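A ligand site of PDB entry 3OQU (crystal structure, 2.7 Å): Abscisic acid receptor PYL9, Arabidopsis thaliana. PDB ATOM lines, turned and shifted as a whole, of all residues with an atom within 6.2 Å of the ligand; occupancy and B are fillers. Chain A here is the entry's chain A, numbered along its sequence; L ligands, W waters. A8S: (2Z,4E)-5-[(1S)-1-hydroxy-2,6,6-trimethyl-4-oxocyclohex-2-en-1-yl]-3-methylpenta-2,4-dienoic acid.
N of Ile 130 lies within hydrogen-bond range of O of Tyr 140, at 2.9 Å. The backbone NH (N) of Val 103 is in hydrogen-bond range of the backbone carbonyl oxygen (O) of Thr 110 (2.9 Å). The side-chain hydroxyl (OG) of Ser 112 lies within hydrogen-bond range of the side-chain carboxylate (OE2) of Glu 114, at 2.8 Å. O of Ser 112 sits at hydrogen-bond distance from N of Val 101 (2.7 Å). O of Leu 137 sits at hydrogen-bond distance from NE2 of His 135. The backbone carbonyl oxygen (O) of Thr 111 is in hydrogen-bond range of a ring nitrogen (ND1) of His 135, 3.4 Å away.
An oxygen (O12) of the ligand lies within salt-bridge range of the side-chain amino group (NZ) of Lys 81, at 2.8 Å. An oxygen (O11) of the ligand sits at hydrogen-bond distance from the side-chain amide nitrogen (ND2) of Asn 187 (2.9 Å).
Merely in contact with the ligand: Phe 83 (3.9 Å), Val 103 (3.7 Å), Ala 109 (3.8 Å), Ser 112 (3.7 Å), Ile 130 (3.8 Å), His 135 (3.8 Å), Leu 137 (3.7 Å), Tyr 140 (3.6 Å), Val 180 (3.9 Å) and Leu 183 (3.5 Å). Hydrophobic or aromatic side chains that line the ligand: Phe 83, Val 103, Ala 109, Ile 130, His 135, Leu 137, Tyr 140, Val 180 and Leu 183. 12 residues have an atom within 4 Å of the ligand: Lys 81, Phe 83, Val 103, Ala 109, Ser 112, Ile 130, His 135, Leu 137, Tyr 140, Val 180, Leu 183 and Asn 187. Along chain A the residues within 4 Å of the ligand span positions 81 to 187. The nearest printed residue that does not touch the ligand is Pro 108 (4.3 Å).
Water W1 lies within hydrogen-bond range of an oxygen (O7) of the ligand (2.7 Å) and the side-chain carboxylate (OE2) of Glu 114 (2.8 Å). Water W4 lies within hydrogen-bond range of the side-chain hydroxyl of Tyr 140, the side-chain carboxylate of Glu 161, an oxygen (O12) of the ligand and the side-chain hydroxyl of Ser 142. Water W3 lies within hydrogen-bond range of the side-chain carboxylate of Glu 161, an oxygen (O12) of the ligand and the side-chain amide nitrogen of Asn 187. Water W2 lies within hydrogen-bond range of an oxygen (O10) of the ligand (2.8 Å), the backbone carbonyl oxygen of Pro 108 (2.9 Å) and the backbone NH of Arg 136 (3.0 Å).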
ATOM      1  N   LYS A  81     -21.853 -21.016   8.139  1.00  0.00           N
ATOM      2  CA  LYS A  81     -21.075 -20.137   9.025  1.00  0.00           C
ATOM      3  C   LYS A  81     -21.739 -20.044  10.400  1.00  0.00           C
ATOM      4  O   LYS A  81     -22.831 -19.502  10.526  1.00  0.00           O
ATOM      5  CB  LYS A  81     -20.887 -18.738   8.415  1.00  0.00           C
ATOM      6  CG  LYS A  81     -20.031 -18.698   7.129  1.00  0.00           C
ATOM      7  CD  LYS A  81     -19.867 -17.273   6.601  1.00  0.00           C
ATOM      8  CE  LYS A  81     -19.224 -17.255   5.210  1.00  0.00           C
ATOM      9  NZ  LYS A  81     -18.580 -15.941   4.865  1.00  0.00           N
ATOM     10  N   PHE A  83     -21.342 -18.380  13.187  1.00  0.00           N
ATOM     11  CA  PHE A  83     -21.472 -17.156  13.981  1.00  0.00           C
ATOM     12  C   PHE A  83     -22.466 -16.134  13.410  1.00  0.00           C
ATOM     13  O   PHE A  83     -22.798 -15.150  14.066  1.00  0.00           O
ATOM     14  CB  PHE A  83     -20.090 -16.523  14.242  1.00  0.00           C
ATOM     15  CG  PHE A  83     -19.134 -17.454  14.951  1.00  0.00           C
ATOM     16  CD1 PHE A  83     -19.446 -17.960  16.208  1.00  0.00           C
ATOM     17  CD2 PHE A  83     -17.925 -17.819  14.355  1.00  0.00           C
ATOM     18  CE1 PHE A  83     -18.560 -18.836  16.864  1.00  0.00           C
ATOM     19  CE2 PHE A  83     -17.044 -18.681  15.004  1.00  0.00           C
ATOM     20  CZ  PHE A  83     -17.356 -19.192  16.249  1.00  0.00           C
ATOM     21  N   VAL A  84     -22.933 -16.379  12.186  1.00  0.00           N
ATOM     22  CA  VAL A  84     -23.925 -15.532  11.535  1.00  0.00           C
ATOM     23  C   VAL A  84     -25.322 -15.873  12.048  1.00  0.00           C
ATOM     24  O   VAL A  84     -25.774 -17.022  11.918  1.00  0.00           O
ATOM     25  CB  VAL A  84     -23.899 -15.724  10.007  1.00  0.00           C
ATOM     26  CG1 VAL A  84     -24.915 -14.803   9.348  1.00  0.00           C
ATOM     27  CG2 VAL A  84     -22.501 -15.470   9.453  1.00  0.00           C
ATOM     28  N   ARG A  99     -24.287  -7.510   1.338  1.00  0.00           N
ATOM     29  CA  ARG A  99     -24.999  -8.232   2.363  1.00  0.00           C
ATOM     30  C   ARG A  99     -24.684  -7.594   3.706  1.00  0.00           C
ATOM     31  O   ARG A  99     -23.553  -7.171   3.939  1.00  0.00           O
ATOM     32  CB  ARG A  99     -24.655  -9.730   2.349  1.00  0.00           C
ATOM     33  CG  ARG A  99     -23.228 -10.133   2.741  1.00  0.00           C
ATOM     34  CD  ARG A  99     -23.067 -11.639   2.653  1.00  0.00           C
ATOM     35  NE  ARG A  99     -21.697 -12.107   2.865  1.00  0.00           N
ATOM     36  CZ  ARG A  99     -21.249 -13.308   2.506  1.00  0.00           C
ATOM     37  NH1 ARG A  99     -22.063 -14.188   1.912  1.00  0.00           N
ATOM     38  NH2 ARG A  99     -19.986 -13.644   2.740  1.00  0.00           N
ATOM     39  N   VAL A 101     -24.504  -8.800   7.436  1.00  0.00           N
ATOM     40  CA  VAL A 101     -24.575  -9.964   8.324  1.00  0.00           C
ATOM     41  C   VAL A 101     -24.616  -9.503   9.763  1.00  0.00           C
ATOM     42  O   VAL A 101     -23.827  -8.656  10.187  1.00  0.00           O
ATOM     43  CB  VAL A 101     -23.467 -11.025   8.062  1.00  0.00           C
ATOM     44  CG1 VAL A 101     -23.259 -11.253   6.565  1.00  0.00           C
ATOM     45  CG2 VAL A 101     -22.160 -10.650   8.728  1.00  0.00           C
ATOM     46  N   VAL A 103     -24.194 -10.847  13.612  1.00  0.00           N
ATOM     47  CA  VAL A 103     -23.349 -11.850  14.213  1.00  0.00           C
ATOM     48  C   VAL A 103     -23.827 -12.172  15.623  1.00  0.00           C
ATOM     49  O   VAL A 103     -24.307 -11.296  16.346  1.00  0.00           O
ATOM     50  CB  VAL A 103     -21.876 -11.374  14.156  1.00  0.00           C
ATOM     51  CG1 VAL A 103     -21.091 -11.781  15.360  1.00  0.00           C
ATOM     52  CG2 VAL A 103     -21.231 -11.903  12.900  1.00  0.00           C
ATOM     53  N   LEU A 107     -18.943 -11.993  20.504  1.00  0.00           N
ATOM     54  CA  LEU A 107     -17.852 -11.620  19.617  1.00  0.00           C
ATOM     55  C   LEU A 107     -17.613 -10.103  19.709  1.00  0.00           C
ATOM     56  O   LEU A 107     -18.516  -9.377  20.141  1.00  0.00           O
ATOM     57  CB  LEU A 107     -18.174 -12.053  18.181  1.00  0.00           C
ATOM     58  CG  LEU A 107     -18.164 -13.577  18.031  1.00  0.00           C
ATOM     59  CD1 LEU A 107     -19.000 -14.052  16.879  1.00  0.00           C
ATOM     60  CD2 LEU A 107     -16.734 -14.094  17.881  1.00  0.00           C
ATOM     61  N   PRO A 108     -16.398  -9.641  19.336  1.00  0.00           N
ATOM     62  CA  PRO A 108     -16.105  -8.194  19.235  1.00  0.00           C
ATOM     63  C   PRO A 108     -16.671  -7.582  17.947  1.00  0.00           C
ATOM     64  O   PRO A 108     -15.941  -6.918  17.191  1.00  0.00           O
ATOM     65  CB  PRO A 108     -14.574  -8.137  19.238  1.00  0.00           C
ATOM     66  CG  PRO A 108     -14.136  -9.464  18.755  1.00  0.00           C
ATOM     67  CD  PRO A 108     -15.188 -10.464  19.121  1.00  0.00           C
ATOM     68  N   ALA A 109     -17.969  -7.796  17.727  1.00  0.00           N
ATOM     69  CA  ALA A 109     -18.661  -7.387  16.522  1.00  0.00           C
ATOM     70  C   ALA A 109     -20.143  -7.684  16.688  1.00  0.00           C
ATOM     71  O   ALA A 109     -20.496  -8.635  17.387  1.00  0.00           O
ATOM     72  CB  ALA A 109     -18.113  -8.137  15.304  1.00  0.00           C
ATOM     73  N   THR A 110     -20.988  -6.872  16.067  1.00  0.00           N
ATOM     74  CA  THR A 110     -22.420  -7.127  16.001  1.00  0.00           C
ATOM     75  C   THR A 110     -22.905  -7.212  14.550  1.00  0.00           C
ATOM     76  O   THR A 110     -23.815  -7.997  14.253  1.00  0.00           O
ATOM     77  CB  THR A 110     -23.259  -6.061  16.752  1.00  0.00           C
ATOM     78  OG1 THR A 110     -23.263  -4.832  15.997  1.00  0.00           O
ATOM     79  CG2 THR A 110     -22.718  -5.831  18.165  1.00  0.00           C
ATOM     80  N   THR A 111     -22.324  -6.400  13.664  1.00  0.00           N
ATOM     81  CA  THR A 111     -22.711  -6.395  12.238  1.00  0.00           C
ATOM     82  C   THR A 111     -21.506  -6.251  11.308  1.00  0.00           C
ATOM     83  O   THR A 111     -20.478  -5.669  11.674  1.00  0.00           O
ATOM     84  CB  THR A 111     -23.710  -5.257  11.871  1.00  0.00           C
ATOM     85  OG1 THR A 111     -23.046  -3.984  11.943  1.00  0.00           O
ATOM     86  CG2 THR A 111     -24.910  -5.231  12.815  1.00  0.00           C
ATOM     87  N   SER A 112     -21.661  -6.767  10.098  1.00  0.00           N
ATOM     88  CA  SER A 112     -20.668  -6.652   9.050  1.00  0.00           C
ATOM     89  C   SER A 112     -21.402  -6.405   7.737  1.00  0.00           C
ATOM     90  O   SER A 112     -22.467  -6.973   7.495  1.00  0.00           O
ATOM     91  CB  SER A 112     -19.869  -7.953   8.963  1.00  0.00           C
ATOM     92  OG  SER A 112     -18.881  -7.887   7.958  1.00  0.00           O
ATOM     93  N   GLU A 114     -20.826  -6.591   3.605  1.00  0.00           N
ATOM     94  CA  GLU A 114     -19.887  -7.313   2.751  1.00  0.00           C
ATOM     95  C   GLU A 114     -20.324  -7.292   1.287  1.00  0.00           C
ATOM     96  O   GLU A 114     -21.508  -7.289   0.992  1.00  0.00           O
ATOM     97  CB  GLU A 114     -19.745  -8.754   3.256  1.00  0.00           C
ATOM     98  CG  GLU A 114     -19.749  -8.843   4.793  1.00  0.00           C
ATOM     99  CD  GLU A 114     -19.489 -10.232   5.338  1.00  0.00           C
ATOM    100  OE1 GLU A 114     -19.747 -11.230   4.634  1.00  0.00           O
ATOM    101  OE2 GLU A 114     -19.013 -10.329   6.497  1.00  0.00           O
ATOM    102  N   ILE A 130     -15.040  -7.242   2.816  1.00  0.00           N
ATOM    103  CA  ILE A 130     -15.757  -6.634   3.940  1.00  0.00           C
ATOM    104  C   ILE A 130     -15.516  -5.132   3.931  1.00  0.00           C
ATOM    105  O   ILE A 130     -14.367  -4.669   4.063  1.00  0.00           O
ATOM    106  CB  ILE A 130     -15.368  -7.268   5.306  1.00  0.00           C
ATOM    107  CG1 ILE A 130     -15.919  -8.703   5.386  1.00  0.00           C
ATOM    108  CG2 ILE A 130     -15.931  -6.421   6.454  1.00  0.00           C
ATOM    109  CD1 ILE A 130     -15.424  -9.482   6.559  1.00  0.00           C
ATOM    110  N   HIS A 135     -16.849  -3.965  13.662  1.00  0.00           N
ATOM    111  CA  HIS A 135     -15.796  -4.904  14.015  1.00  0.00           C
ATOM    112  C   HIS A 135     -14.414  -4.350  13.682  1.00  0.00           C
ATOM    113  O   HIS A 135     -14.287  -3.265  13.095  1.00  0.00           O
ATOM    114  CB  HIS A 135     -16.015  -6.212  13.256  1.00  0.00           C
ATOM    115  CG  HIS A 135     -16.008  -6.045  11.778  1.00  0.00           C
ATOM    116  ND1 HIS A 135     -17.169  -5.983  11.030  1.00  0.00           N
ATOM    117  CD2 HIS A 135     -14.989  -5.897  10.900  1.00  0.00           C
ATOM    118  CE1 HIS A 135     -16.861  -5.817   9.753  1.00  0.00           C
ATOM    119  NE2 HIS A 135     -15.546  -5.754   9.646  1.00  0.00           N
ATOM    120  N   ARG A 136     -13.379  -5.115  14.016  1.00  0.00           N
ATOM    121  CA  ARG A 136     -12.008  -4.626  13.908  1.00  0.00           C
ATOM    122  C   ARG A 136     -11.219  -5.149  12.703  1.00  0.00           C
ATOM    123  O   ARG A 136      -9.986  -5.207  12.737  1.00  0.00           O
ATOM    124  CB  ARG A 136     -11.261  -4.834  15.243  1.00  0.00           C
ATOM    125  CG  ARG A 136     -11.292  -6.250  15.807  1.00  0.00           C
ATOM    126  CD  ARG A 136     -10.738  -6.351  17.228  1.00  0.00           C
ATOM    127  NE  ARG A 136     -11.605  -5.716  18.226  1.00  0.00           N
ATOM    128  CZ  ARG A 136     -11.700  -6.081  19.510  1.00  0.00           C
ATOM    129  NH1 ARG A 136     -10.974  -7.094  19.969  1.00  0.00           N
ATOM    130  NH2 ARG A 136     -12.516  -5.435  20.342  1.00  0.00           N
ATOM    131  N   LEU A 137     -11.929  -5.507  11.633  1.00  0.00           N
ATOM    132  CA  LEU A 137     -11.294  -5.989  10.403  1.00  0.00           C
ATOM    133  C   LEU A 137     -11.464  -5.003   9.244  1.00  0.00           C
ATOM    134  O   LEU A 137     -12.387  -5.134   8.439  1.00  0.00           O
ATOM    135  CB  LEU A 137     -11.850  -7.359   9.989  1.00  0.00           C
ATOM    136  CG  LEU A 137     -11.816  -8.565  10.933  1.00  0.00           C
ATOM    137  CD1 LEU A 137     -12.220  -9.796  10.164  1.00  0.00           C
ATOM    138  CD2 LEU A 137     -10.441  -8.768  11.563  1.00  0.00           C
ATOM    139  N   TYR A 140     -10.586  -6.122   4.788  1.00  0.00           N
ATOM    140  CA  TYR A 140     -10.640  -7.567   4.659  1.00  0.00           C
ATOM    141  C   TYR A 140     -11.084  -7.984   3.270  1.00  0.00           C
ATOM    142  O   TYR A 140     -12.150  -7.586   2.796  1.00  0.00           O
ATOM    143  CB  TYR A 140     -11.610  -8.164   5.670  1.00  0.00           C
ATOM    144  CG  TYR A 140     -11.677  -9.671   5.635  1.00  0.00           C
ATOM    145  CD1 TYR A 140     -10.894 -10.440   6.499  1.00  0.00           C
ATOM    146  CD2 TYR A 140     -12.521 -10.324   4.748  1.00  0.00           C
ATOM    147  CE1 TYR A 140     -10.948 -11.827   6.477  1.00  0.00           C
ATOM    148  CE2 TYR A 140     -12.602 -11.693   4.711  1.00  0.00           C
ATOM    149  CZ  TYR A 140     -11.812 -12.441   5.574  1.00  0.00           C
ATOM    150  OH  TYR A 140     -11.899 -13.809   5.528  1.00  0.00           O
ATOM    151  N   SER A 142     -11.274 -11.497   0.645  1.00  0.00           N
ATOM    152  CA  SER A 142     -11.336 -12.946   0.763  1.00  0.00           C
ATOM    153  C   SER A 142     -11.426 -13.609  -0.600  1.00  0.00           C
ATOM    154  O   SER A 142     -12.134 -13.127  -1.491  1.00  0.00           O
ATOM    155  CB  SER A 142     -12.547 -13.319   1.596  1.00  0.00           C
ATOM    156  OG  SER A 142     -12.603 -14.711   1.828  1.00  0.00           O
ATOM    157  N   GLU A 161      -9.473 -21.263   1.365  1.00  0.00           N
ATOM    158  CA  GLU A 161      -9.893 -19.871   1.568  1.00  0.00           C
ATOM    159  C   GLU A 161      -8.747 -19.067   2.148  1.00  0.00           C
ATOM    160  O   GLU A 161      -8.164 -19.444   3.163  1.00  0.00           O
ATOM    161  CB  GLU A 161     -11.134 -19.767   2.479  1.00  0.00           C
ATOM    162  CG  GLU A 161     -11.526 -18.320   2.843  1.00  0.00           C
ATOM    163  CD  GLU A 161     -12.949 -18.155   3.376  1.00  0.00           C
ATOM    164  OE1 GLU A 161     -13.425 -19.013   4.136  1.00  0.00           O
ATOM    165  OE2 GLU A 161     -13.604 -17.147   3.026  1.00  0.00           O
ATOM    166  N   VAL A 180      -8.195 -14.217  12.892  1.00  0.00           N
ATOM    167  CA  VAL A 180      -9.005 -14.388  11.690  1.00  0.00           C
ATOM    168  C   VAL A 180      -8.982 -15.855  11.264  1.00  0.00           C
ATOM    169  O   VAL A 180     -10.043 -16.404  10.877  1.00  0.00           O
ATOM    170  CB  VAL A 180      -8.541 -13.455  10.539  1.00  0.00           C
ATOM    171  CG1 VAL A 180      -9.387 -13.668   9.294  1.00  0.00           C
ATOM    172  CG2 VAL A 180      -8.617 -12.008  10.973  1.00  0.00           C
ATOM    173  N   LEU A 183     -11.602 -17.921  13.003  1.00  0.00           N
ATOM    174  CA  LEU A 183     -12.905 -17.767  12.377  1.00  0.00           C
ATOM    175  C   LEU A 183     -13.045 -18.621  11.123  1.00  0.00           C
ATOM    176  O   LEU A 183     -14.088 -19.266  10.914  1.00  0.00           O
ATOM    177  CB  LEU A 183     -13.161 -16.301  12.060  1.00  0.00           C
ATOM    178  CG  LEU A 183     -13.181 -15.431  13.315  1.00  0.00           C
ATOM    179  CD1 LEU A 183     -13.192 -13.957  12.934  1.00  0.00           C
ATOM    180  CD2 LEU A 183     -14.365 -15.795  14.228  1.00  0.00           C
ATOM    181  N   ILE A 184     -12.009 -18.637  10.290  1.00  0.00           N
ATOM    182  CA  ILE A 184     -12.107 -19.364   9.030  1.00  0.00           C
ATOM    183  C   ILE A 184     -12.123 -20.890   9.225  1.00  0.00           C
ATOM    184  O   ILE A 184     -12.879 -21.599   8.561  1.00  0.00           O
ATOM    185  CB  ILE A 184     -11.072 -18.860   7.997  1.00  0.00           C
ATOM    186  CG1 ILE A 184     -11.340 -17.374   7.740  1.00  0.00           C
ATOM    187  CG2 ILE A 184     -11.173 -19.654   6.703  1.00  0.00           C
ATOM    188  CD1 ILE A 184     -10.504 -16.730   6.656  1.00  0.00           C
ATOM    189  N   ASN A 187     -15.649 -21.739  10.174  1.00  0.00           N
ATOM    190  CA  ASN A 187     -16.483 -21.750   8.968  1.00  0.00           C
ATOM    191  C   ASN A 187     -16.264 -22.981   8.078  1.00  0.00           C
ATOM    192  O   ASN A 187     -17.243 -23.625   7.669  1.00  0.00           O
ATOM    193  CB  ASN A 187     -16.290 -20.453   8.156  1.00  0.00           C
ATOM    194  CG  ASN A 187     -16.763 -19.195   8.904  1.00  0.00           C
ATOM    195  OD1 ASN A 187     -17.553 -19.266   9.850  1.00  0.00           O
ATOM    196  ND2 ASN A 187     -16.293 -18.021   8.457  1.00  0.00           N
HETATM  197  C1  A8S L   1     -16.013 -15.043   7.163  1.00  0.00           C
HETATM  198  C2  A8S L   1     -14.709 -14.523   7.662  1.00  0.00           C
HETATM  199  C3  A8S L   1     -14.593 -13.763   8.771  1.00  0.00           C
HETATM  200  C4  A8S L   1     -15.785 -13.392   9.587  1.00  0.00           C
HETATM  201  C5  A8S L   1     -15.685 -12.419  10.500  1.00  0.00           C
HETATM  202  C6  A8S L   1     -13.237 -13.274   9.206  1.00  0.00           C
HETATM  203  C7  A8S L   1     -16.857 -11.982  11.350  1.00  0.00           C
HETATM  204  O7  A8S L   1     -18.085 -12.374  10.714  1.00  0.00           O
HETATM  205  C8  A8S L   1     -16.768 -12.709  12.692  1.00  0.00           C
HETATM  206  C9  A8S L   1     -16.127 -12.159  13.744  1.00  0.00           C
HETATM  207  C10 A8S L   1     -15.573 -10.770  13.690  1.00  0.00           C
HETATM  208  O10 A8S L   1     -14.963 -10.313  14.650  1.00  0.00           O
HETATM  209  C11 A8S L   1     -15.756  -9.936  12.441  1.00  0.00           C
HETATM  210  O11 A8S L   1     -16.975 -15.262   7.955  1.00  0.00           O
HETATM  211  C12 A8S L   1     -16.832 -10.452  11.489  1.00  0.00           C
HETATM  212  O12 A8S L   1     -16.136 -15.258   5.935  1.00  0.00           O
HETATM  213  C13 A8S L   1     -17.409 -14.057  12.859  1.00  0.00           C
HETATM  214  C14 A8S L   1     -16.588  -9.767  10.150  1.00  0.00           C
HETATM  215  C15 A8S L   1     -18.212 -10.005  11.982  1.00  0.00           C
HETATM  216  O   HOH W   1     -18.874 -12.554   8.177  1.00  0.00           O
HETATM  217  O   HOH W   2     -13.913  -7.785  15.373  1.00  0.00           O
HETATM  218  O   HOH W   3     -15.228 -17.900   5.508  1.00  0.00           O
HETATM  219  O   HOH W   4     -13.974 -14.860   4.320  1.00  0.00           O
HETATM  220  O   HOH W   5     -19.016 -15.179   9.876  1.00  0.00           O
